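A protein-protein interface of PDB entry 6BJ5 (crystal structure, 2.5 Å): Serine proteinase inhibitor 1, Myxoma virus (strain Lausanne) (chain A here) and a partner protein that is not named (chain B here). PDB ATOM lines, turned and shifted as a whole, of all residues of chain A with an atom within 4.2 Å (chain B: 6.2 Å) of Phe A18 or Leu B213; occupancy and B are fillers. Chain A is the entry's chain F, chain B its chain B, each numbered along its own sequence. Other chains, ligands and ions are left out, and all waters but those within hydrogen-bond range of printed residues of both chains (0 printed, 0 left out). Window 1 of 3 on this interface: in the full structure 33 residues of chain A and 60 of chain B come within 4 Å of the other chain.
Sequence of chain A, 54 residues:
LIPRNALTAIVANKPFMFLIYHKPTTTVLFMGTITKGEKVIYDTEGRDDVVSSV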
ATOM      1  N   MET A  17      18.068  23.399 -14.715  1.00  0.00           N
ATOM      2  CA  MET A  17      17.516  24.617 -14.144  1.00  0.00           C
ATOM      3  C   MET A  17      16.023  24.680 -14.437  1.00  0.00           C
ATOM      4  O   MET A  17      15.578  24.280 -15.519  1.00  0.00           O
ATOM      5  CB  MET A  17      18.227  25.866 -14.714  1.00  0.00           C
ATOM      6  CG  MET A  17      17.601  27.176 -14.267  1.00  0.00           C
ATOM      7  SD  MET A  17      18.423  28.649 -14.890  1.00  0.00           S
ATOM      8  CE  MET A  17      19.830  28.750 -13.805  1.00  0.00           C
ATOM      9  N   PHE A  18      15.243  25.179 -13.477  1.00  0.00           N
ATOM     10  CA  PHE A  18      13.845  25.452 -13.759  1.00  0.00           C
ATOM     11  C   PHE A  18      13.507  26.872 -13.321  1.00  0.00           C
ATOM     12  O   PHE A  18      14.116  27.430 -12.403  1.00  0.00           O
ATOM     13  CB  PHE A  18      12.904  24.429 -13.101  1.00  0.00           C
ATOM     14  CG  PHE A  18      12.919  24.487 -11.615  1.00  0.00           C
ATOM     15  CD1 PHE A  18      12.068  25.337 -10.940  1.00  0.00           C
ATOM     16  CD2 PHE A  18      13.810  23.722 -10.895  1.00  0.00           C
ATOM     17  CE1 PHE A  18      12.107  25.423  -9.592  1.00  0.00           C
ATOM     18  CE2 PHE A  18      13.843  23.810  -9.547  1.00  0.00           C
ATOM     19  CZ  PHE A  18      12.996  24.665  -8.888  1.00  0.00           C
ATOM     20  N   LEU A  19      12.515  27.440 -13.997  1.00  0.00           N
ATOM     21  CA  LEU A  19      12.040  28.795 -13.768  1.00  0.00           C
ATOM     22  C   LEU A  19      10.529  28.693 -13.790  1.00  0.00           C
ATOM     23  O   LEU A  19       9.962  28.175 -14.756  1.00  0.00           O
ATOM     24  CB  LEU A  19      12.523  29.729 -14.876  1.00  0.00           C
ATOM     25  CG  LEU A  19      14.037  29.771 -15.064  1.00  0.00           C
ATOM     26  CD1 LEU A  19      14.333  29.548 -16.520  1.00  0.00           C
ATOM     27  CD2 LEU A  19      14.540  31.102 -14.679  1.00  0.00           C
ATOM     28  N   TYR A  21       7.394  31.011 -13.969  1.00  0.00           N
ATOM     29  CA  TYR A  21       7.167  32.393 -14.368  1.00  0.00           C
ATOM     30  C   TYR A  21       5.690  32.622 -14.674  1.00  0.00           C
ATOM     31  O   TYR A  21       4.933  31.684 -14.948  1.00  0.00           O
ATOM     32  CB  TYR A  21       8.053  32.776 -15.573  1.00  0.00           C
ATOM     33  CG  TYR A  21       7.517  32.412 -16.938  1.00  0.00           C
ATOM     34  CD1 TYR A  21       6.965  33.384 -17.763  1.00  0.00           C
ATOM     35  CD2 TYR A  21       7.610  31.117 -17.427  1.00  0.00           C
ATOM     36  CE1 TYR A  21       6.484  33.073 -19.027  1.00  0.00           C
ATOM     37  CE2 TYR A  21       7.129  30.788 -18.686  1.00  0.00           C
ATOM     38  CZ  TYR A  21       6.562  31.775 -19.487  1.00  0.00           C
ATOM     39  OH  TYR A  21       6.071  31.473 -20.746  1.00  0.00           O
ATOM     40  N   MET A  31      12.629  30.020  -9.059  1.00  0.00           N
ATOM     41  CA  MET A  31      13.731  29.444  -9.799  1.00  0.00           C
ATOM     42  C   MET A  31      14.413  28.407  -8.934  1.00  0.00           C
ATOM     43  O   MET A  31      14.361  28.465  -7.701  1.00  0.00           O
ATOM     44  CB  MET A  31      14.842  30.432 -10.081  1.00  0.00           C
ATOM     45  CG  MET A  31      14.648  31.537 -11.006  1.00  0.00           C
ATOM     46  SD  MET A  31      16.278  32.281 -10.811  1.00  0.00           S
ATOM     47  CE  MET A  31      17.299  31.165 -11.777  1.00  0.00           C
ATOM     48  N   GLY A  32      15.160  27.531  -9.597  1.00  0.00           N
ATOM     49  CA  GLY A  32      16.057  26.655  -8.879  1.00  0.00           C
ATOM     50  C   GLY A  32      16.959  25.884  -9.811  1.00  0.00           C
ATOM     51  O   GLY A  32      16.672  25.732 -11.003  1.00  0.00           O
ATOM     52  N   ILE A  34      18.946  22.031  -9.860  1.00  0.00           N
ATOM     53  CA  ILE A  34      18.952  20.684  -9.306  1.00  0.00           C
ATOM     54  C   ILE A  34      20.187  19.955  -9.827  1.00  0.00           C
ATOM     55  O   ILE A  34      20.242  19.588 -11.006  1.00  0.00           O
ATOM     56  CB  ILE A  34      17.658  19.962  -9.672  1.00  0.00           C
ATOM     57  CG1 ILE A  34      16.541  20.624  -8.900  1.00  0.00           C
ATOM     58  CG2 ILE A  34      17.719  18.502  -9.364  1.00  0.00           C
ATOM     59  CD1 ILE A  34      15.251  20.156  -9.346  1.00  0.00           C
ATOM     60  N   VAL B  33      19.407  24.268  -5.081  1.00  0.00           N
ATOM     61  CA  VAL B  33      19.038  25.578  -4.572  1.00  0.00           C
ATOM     62  C   VAL B  33      17.749  26.014  -5.246  1.00  0.00           C
ATOM     63  O   VAL B  33      17.602  25.866  -6.464  1.00  0.00           O
ATOM     64  CB  VAL B  33      20.149  26.609  -4.824  1.00  0.00           C
ATOM     65  CG1 VAL B  33      19.740  27.978  -4.288  1.00  0.00           C
ATOM     66  CG2 VAL B  33      21.449  26.134  -4.213  1.00  0.00           C
ATOM     67  N   VAL B  34      16.819  26.536  -4.452  1.00  0.00           N
ATOM     68  CA  VAL B  34      15.580  27.122  -4.942  1.00  0.00           C
ATOM     69  C   VAL B  34      15.493  28.558  -4.436  1.00  0.00           C
ATOM     70  O   VAL B  34      16.000  28.904  -3.363  1.00  0.00           O
ATOM     71  CB  VAL B  34      14.351  26.297  -4.517  1.00  0.00           C
ATOM     72  CG1 VAL B  34      14.464  24.893  -5.076  1.00  0.00           C
ATOM     73  CG2 VAL B  34      14.249  26.250  -3.012  1.00  0.00           C
ATOM     74  N   VAL B 200      15.324  24.230 -23.798  1.00  0.00           N
ATOM     75  CA  VAL B 200      14.375  24.876 -22.902  1.00  0.00           C
ATOM     76  C   VAL B 200      12.994  24.385 -23.300  1.00  0.00           C
ATOM     77  O   VAL B 200      12.675  24.316 -24.491  1.00  0.00           O
ATOM     78  CB  VAL B 200      14.461  26.417 -22.965  1.00  0.00           C
ATOM     79  CG1 VAL B 200      13.470  27.058 -22.009  1.00  0.00           C
ATOM     80  CG2 VAL B 200      15.866  26.888 -22.655  1.00  0.00           C
ATOM     81  N   THR B 201      12.187  24.015 -22.311  1.00  0.00           N
ATOM     82  CA  THR B 201      10.902  23.388 -22.563  1.00  0.00           C
ATOM     83  C   THR B 201       9.879  23.971 -21.601  1.00  0.00           C
ATOM     84  O   THR B 201      10.148  24.079 -20.404  1.00  0.00           O
ATOM     85  CB  THR B 201      11.016  21.863 -22.381  1.00  0.00           C
ATOM     86  OG1 THR B 201      12.034  21.348 -23.257  1.00  0.00           O
ATOM     87  CG2 THR B 201       9.682  21.172 -22.647  1.00  0.00           C
ATOM     88  N   GLU B 202       8.691  24.295 -22.106  1.00  0.00           N
ATOM     89  CA  GLU B 202       7.677  24.965 -21.304  1.00  0.00           C
ATOM     90  C   GLU B 202       6.611  23.971 -20.880  1.00  0.00           C
ATOM     91  O   GLU B 202       5.841  23.474 -21.704  1.00  0.00           O
ATOM     92  CB  GLU B 202       7.055  26.143 -22.061  1.00  0.00           C
ATOM     93  CG  GLU B 202       6.140  26.923 -21.148  1.00  0.00           C
ATOM     94  CD  GLU B 202       5.691  28.243 -21.694  1.00  0.00           C
ATOM     95  OE1 GLU B 202       6.559  29.061 -22.072  1.00  0.00           O
ATOM     96  OE2 GLU B 202       4.476  28.495 -21.661  1.00  0.00           O
ATOM     97  N   LEU B 203       6.537  23.732 -19.588  1.00  0.00           N
ATOM     98  CA  LEU B 203       5.511  22.896 -18.993  1.00  0.00           C
ATOM     99  C   LEU B 203       4.433  23.797 -18.426  1.00  0.00           C
ATOM    100  O   LEU B 203       4.652  24.434 -17.389  1.00  0.00           O
ATOM    101  CB  LEU B 203       6.116  22.028 -17.892  1.00  0.00           C
ATOM    102  CG  LEU B 203       7.333  21.199 -18.279  1.00  0.00           C
ATOM    103  CD1 LEU B 203       8.034  20.747 -17.019  1.00  0.00           C
ATOM    104  CD2 LEU B 203       6.880  19.992 -19.064  1.00  0.00           C
ATOM    105  N   ALA B 211       3.809  28.869 -15.703  1.00  0.00           N
ATOM    106  CA  ALA B 211       4.377  27.722 -16.398  1.00  0.00           C
ATOM    107  C   ALA B 211       5.800  27.489 -15.918  1.00  0.00           C
ATOM    108  O   ALA B 211       6.459  28.402 -15.411  1.00  0.00           O
ATOM    109  CB  ALA B 211       4.351  27.938 -17.914  1.00  0.00           C
ATOM    110  N   MET B 212       6.292  26.276 -16.146  1.00  0.00           N
ATOM    111  CA  MET B 212       7.664  25.939 -15.802  1.00  0.00           C
ATOM    112  C   MET B 212       8.500  25.850 -17.065  1.00  0.00           C
ATOM    113  O   MET B 212       8.150  25.137 -18.006  1.00  0.00           O
ATOM    114  CB  MET B 212       7.761  24.643 -14.998  1.00  0.00           C
ATOM    115  CG  MET B 212       9.208  24.271 -14.688  1.00  0.00           C
ATOM    116  SD  MET B 212       9.453  22.856 -13.592  1.00  0.00           S
ATOM    117  CE  MET B 212       9.073  23.608 -12.007  1.00  0.00           C
ATOM    118  N   LEU B 213       9.571  26.615 -17.091  1.00  0.00           N
ATOM    119  CA  LEU B 213      10.601  26.476 -18.096  1.00  0.00           C
ATOM    120  C   LEU B 213      11.616  25.509 -17.527  1.00  0.00           C
ATOM    121  O   LEU B 213      12.130  25.723 -16.423  1.00  0.00           O
ATOM    122  CB  LEU B 213      11.242  27.827 -18.413  1.00  0.00           C
ATOM    123  CG  LEU B 213      10.274  28.894 -18.945  1.00  0.00           C
ATOM    124  CD1 LEU B 213      11.006  30.186 -19.161  1.00  0.00           C
ATOM    125  CD2 LEU B 213       9.590  28.434 -20.238  1.00  0.00           C
ATOM    126  N   LEU B 214      11.873  24.436 -18.259  1.00  0.00           N
ATOM    127  CA  LEU B 214      12.861  23.445 -17.879  1.00  0.00           C
ATOM    128  C   LEU B 214      14.036  23.603 -18.843  1.00  0.00           C
ATOM    129  O   LEU B 214      13.855  23.571 -20.068  1.00  0.00           O
ATOM    130  CB  LEU B 214      12.241  22.054 -17.910  1.00  0.00           C
ATOM    131  CG  LEU B 214      13.133  20.812 -17.765  1.00  0.00           C
ATOM    132  CD1 LEU B 214      13.672  20.682 -16.345  1.00  0.00           C
ATOM    133  CD2 LEU B 214      12.378  19.567 -18.153  1.00  0.00           C
ATOM    134  N   VAL B 215      15.212  23.832 -18.282  1.00  0.00           N
ATOM    135  CA  VAL B 215      16.451  24.133 -18.982  1.00  0.00           C
ATOM    136  C   VAL B 215      17.409  22.978 -18.727  1.00  0.00           C
ATOM    137  O   VAL B 215      17.837  22.779 -17.581  1.00  0.00           O
ATOM    138  CB  VAL B 215      17.047  25.462 -18.481  1.00  0.00           C
ATOM    139  CG1 VAL B 215      18.344  25.835 -19.228  1.00  0.00           C
ATOM    140  CG2 VAL B 215      16.010  26.589 -18.587  1.00  0.00           C
ATOM    141  N   VAL B 232      15.639  35.131 -21.098  1.00  0.00           N
ATOM    142  CA  VAL B 232      14.366  34.446 -20.875  1.00  0.00           C
ATOM    143  C   VAL B 232      13.365  34.784 -21.970  1.00  0.00           C
ATOM    144  O   VAL B 232      12.670  33.901 -22.486  1.00  0.00           O
ATOM    145  CB  VAL B 232      13.807  34.767 -19.480  1.00  0.00           C
ATOM    146  CG1 VAL B 232      12.407  34.216 -19.355  1.00  0.00           C
ATOM    147  CG2 VAL B 232      14.711  34.173 -18.409  1.00  0.00           C
ATOM    148  N   TRP B 235      14.344  32.926 -25.045  1.00  0.00           N
ATOM    149  CA  TRP B 235      13.813  31.572 -24.938  1.00  0.00           C
ATOM    150  C   TRP B 235      12.350  31.531 -25.335  1.00  0.00           C
ATOM    151  O   TRP B 235      11.945  30.687 -26.133  1.00  0.00           O
ATOM    152  CB  TRP B 235      13.980  31.034 -23.514  1.00  0.00           C
ATOM    153  CG  TRP B 235      15.383  30.747 -23.120  1.00  0.00           C
ATOM    154  CD1 TRP B 235      16.453  30.583 -23.954  1.00  0.00           C
ATOM    155  CD2 TRP B 235      15.885  30.613 -21.785  1.00  0.00           C
ATOM    156  NE1 TRP B 235      17.583  30.340 -23.221  1.00  0.00           N
ATOM    157  CE2 TRP B 235      17.266  30.355 -21.885  1.00  0.00           C
ATOM    158  CE3 TRP B 235      15.297  30.674 -20.514  1.00  0.00           C
ATOM    159  CZ2 TRP B 235      18.082  30.154 -20.756  1.00  0.00           C
ATOM    160  CZ3 TRP B 235      16.116  30.488 -19.379  1.00  0.00           C
ATOM    161  CH2 TRP B 235      17.490  30.232 -19.514  1.00  0.00           C
ATOM    162  N   ILE B 236      11.535  32.443 -24.791  1.00  0.00           N
ATOM    163  CA  ILE B 236      10.104  32.333 -25.052  1.00  0.00           C
ATOM    164  C   ILE B 236       9.795  32.582 -26.522  1.00  0.00           C
ATOM    165  O   ILE B 236       8.871  31.972 -27.080  1.00  0.00           O
ATOM    166  CB  ILE B 236       9.313  33.266 -24.126  1.00  0.00           C
ATOM    167  CG1 ILE B 236       9.420  32.751 -22.685  1.00  0.00           C
ATOM    168  CG2 ILE B 236       7.845  33.353 -24.591  1.00  0.00           C
ATOM    169  CD1 ILE B 236       8.875  33.678 -21.636  1.00  0.00           C
ATOM    170  N   MET B 239      11.319  29.279 -28.693  1.00  0.00           N
ATOM    171  CA  MET B 239      10.823  27.922 -28.507  1.00  0.00           C
ATOM    172  C   MET B 239       9.675  27.696 -29.472  1.00  0.00           C
ATOM    173  O   MET B 239       8.855  28.589 -29.699  1.00  0.00           O
ATOM    174  CB  MET B 239      10.356  27.664 -27.073  1.00  0.00           C
ATOM    175  CG  MET B 239      11.444  27.716 -26.021  1.00  0.00           C
ATOM    176  SD  MET B 239      10.755  27.346 -24.399  1.00  0.00           S
ATOM    177  CE  MET B 239       9.583  28.681 -24.158  1.00  0.00           C
ATOM    178  N   MET B 248      11.664  13.648 -16.402  1.00  0.00           N
ATOM    179  CA  MET B 248      12.255  14.538 -15.419  1.00  0.00           C
ATOM    180  C   MET B 248      11.944  14.031 -14.033  1.00  0.00           C
ATOM    181  O   MET B 248      10.915  13.366 -13.817  1.00  0.00           O
ATOM    182  CB  MET B 248      11.745  15.978 -15.604  1.00  0.00           C
ATOM    183  CG  MET B 248      10.350  16.199 -15.093  1.00  0.00           C
ATOM    184  SD  MET B 248       9.846  17.922 -15.224  1.00  0.00           S
ATOM    185  CE  MET B 248      11.047  18.752 -14.205  1.00  0.00           C
ATOM    186  N   PHE B 251      10.967  16.239  -7.507  1.00  0.00           N
ATOM    187  CA  PHE B 251      11.924  16.837  -6.589  1.00  0.00           C
ATOM    188  C   PHE B 251      11.224  17.681  -5.536  1.00  0.00           C
ATOM    189  O   PHE B 251      10.147  18.253  -5.758  1.00  0.00           O
ATOM    190  CB  PHE B 251      12.989  17.657  -7.323  1.00  0.00           C
ATOM    191  CG  PHE B 251      12.458  18.813  -8.116  1.00  0.00           C
ATOM    192  CD1 PHE B 251      12.257  20.054  -7.516  1.00  0.00           C
ATOM    193  CD2 PHE B 251      12.191  18.673  -9.473  1.00  0.00           C
ATOM    194  CE1 PHE B 251      11.785  21.143  -8.267  1.00  0.00           C
ATOM    195  CE2 PHE B 251      11.718  19.749 -10.221  1.00  0.00           C
ATOM    196  CZ  PHE B 251      11.513  20.991  -9.602  1.00  0.00           C
ATOM    197  N   ILE B 299      10.265  24.246  -2.898  1.00  0.00           N
ATOM    198  CA  ILE B 299       9.591  23.910  -4.150  1.00  0.00           C
ATOM    199  C   ILE B 299       9.418  22.399  -4.183  1.00  0.00           C
ATOM    200  O   ILE B 299      10.326  21.650  -3.793  1.00  0.00           O
ATOM    201  CB  ILE B 299      10.355  24.421  -5.403  1.00  0.00           C
ATOM    202  CG1 ILE B 299      10.505  25.947  -5.339  1.00  0.00           C
ATOM    203  CG2 ILE B 299       9.585  24.118  -6.694  1.00  0.00           C
ATOM    204  CD1 ILE B 299      11.359  26.560  -6.399  1.00  0.00           C
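OH of Tyr A21 lies within hydrogen-bond range of OE1 of Glu B202 (2.8 Å). N of Ala B211 is in hydrogen-bond range of O of Tyr A21. The backbone carbonyl oxygen of Met A17 is in hydrogen-bond range of the backbone NH of Val B215, at 2.8 Å. The backbone carbonyl oxygen (O) of Leu A19 sits at hydrogen-bond distance from the backbone NH (N) of Leu B213.
O of Thr B201 lies within hydrogen-bond range of N of Leu B214, 2.8 Å away. The backbone NH (N) of Leu B203 is in hydrogen-bond range of the backbone carbonyl oxygen (O) of Met B212, 2.7 Å away. The backbone NH (N) of Phe A18 is in hydrogen-bond range of the backbone carbonyl oxygen (O) of Gly A32 (2.9 Å).
CA of Leu B214 touches O of Met A17 (3.7 Å). Phe A18 touches Met B212 (CD1 to CE, 3.6 Å). Phe A18 touches Leu B213. Leu A19 touches Met B212. Val B215 touches Leu A19. CD1 of Leu A19 touches CZ3 of Trp B235 (3.5 Å). Tyr A21 touches Leu B213 (CE2 to CG, 3.7 Å). O of Met A31 touches CA of Val B34, at 3.3 Å. Val B34 touches Gly A32. CD1 of Ile A34 touches CG of Phe B251, at 3.3 Å.
Of chain A, only Met A17 (3.8 Å), Phe A18 (3.2 Å), Leu A19 (2.8 Å) and Tyr A21 (3.7 Å) come within 4 Å of Leu B213. Printed residues of chain B within 4 Å of Gly A32: Val B33 (3.0 Å) and Val B34 (3.99 Å). Of the printed residues of chain A, Val B33 touches Gly A32 (3.0 Å). Of the printed residues of chain A, Phe B251 touches Phe A18 and Ile A34. Leu B203 touches none of the printed residues of chain A. Met B239 touches none of the printed residues of chain A. The nearest printed residue of chain A that does not touch Leu B213 is Gly A32 (7.1 Å). The nearest printed residue of chain A that does not touch Ile B236 is Leu A19 (8.5 Å).
Of the 18 printed residues of chain B, 12 touch a printed residue of chain A. Hydrophobic or aromatic side chains of chain B within 4 Å of the printed part of chain A: Val B34, Met B212, Leu B213, Val B215, Trp B235, Ile B236, Phe B251 and Ile B299. Along chain A the printed residues that touch a printed residue of chain B span positions 17 to 34.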
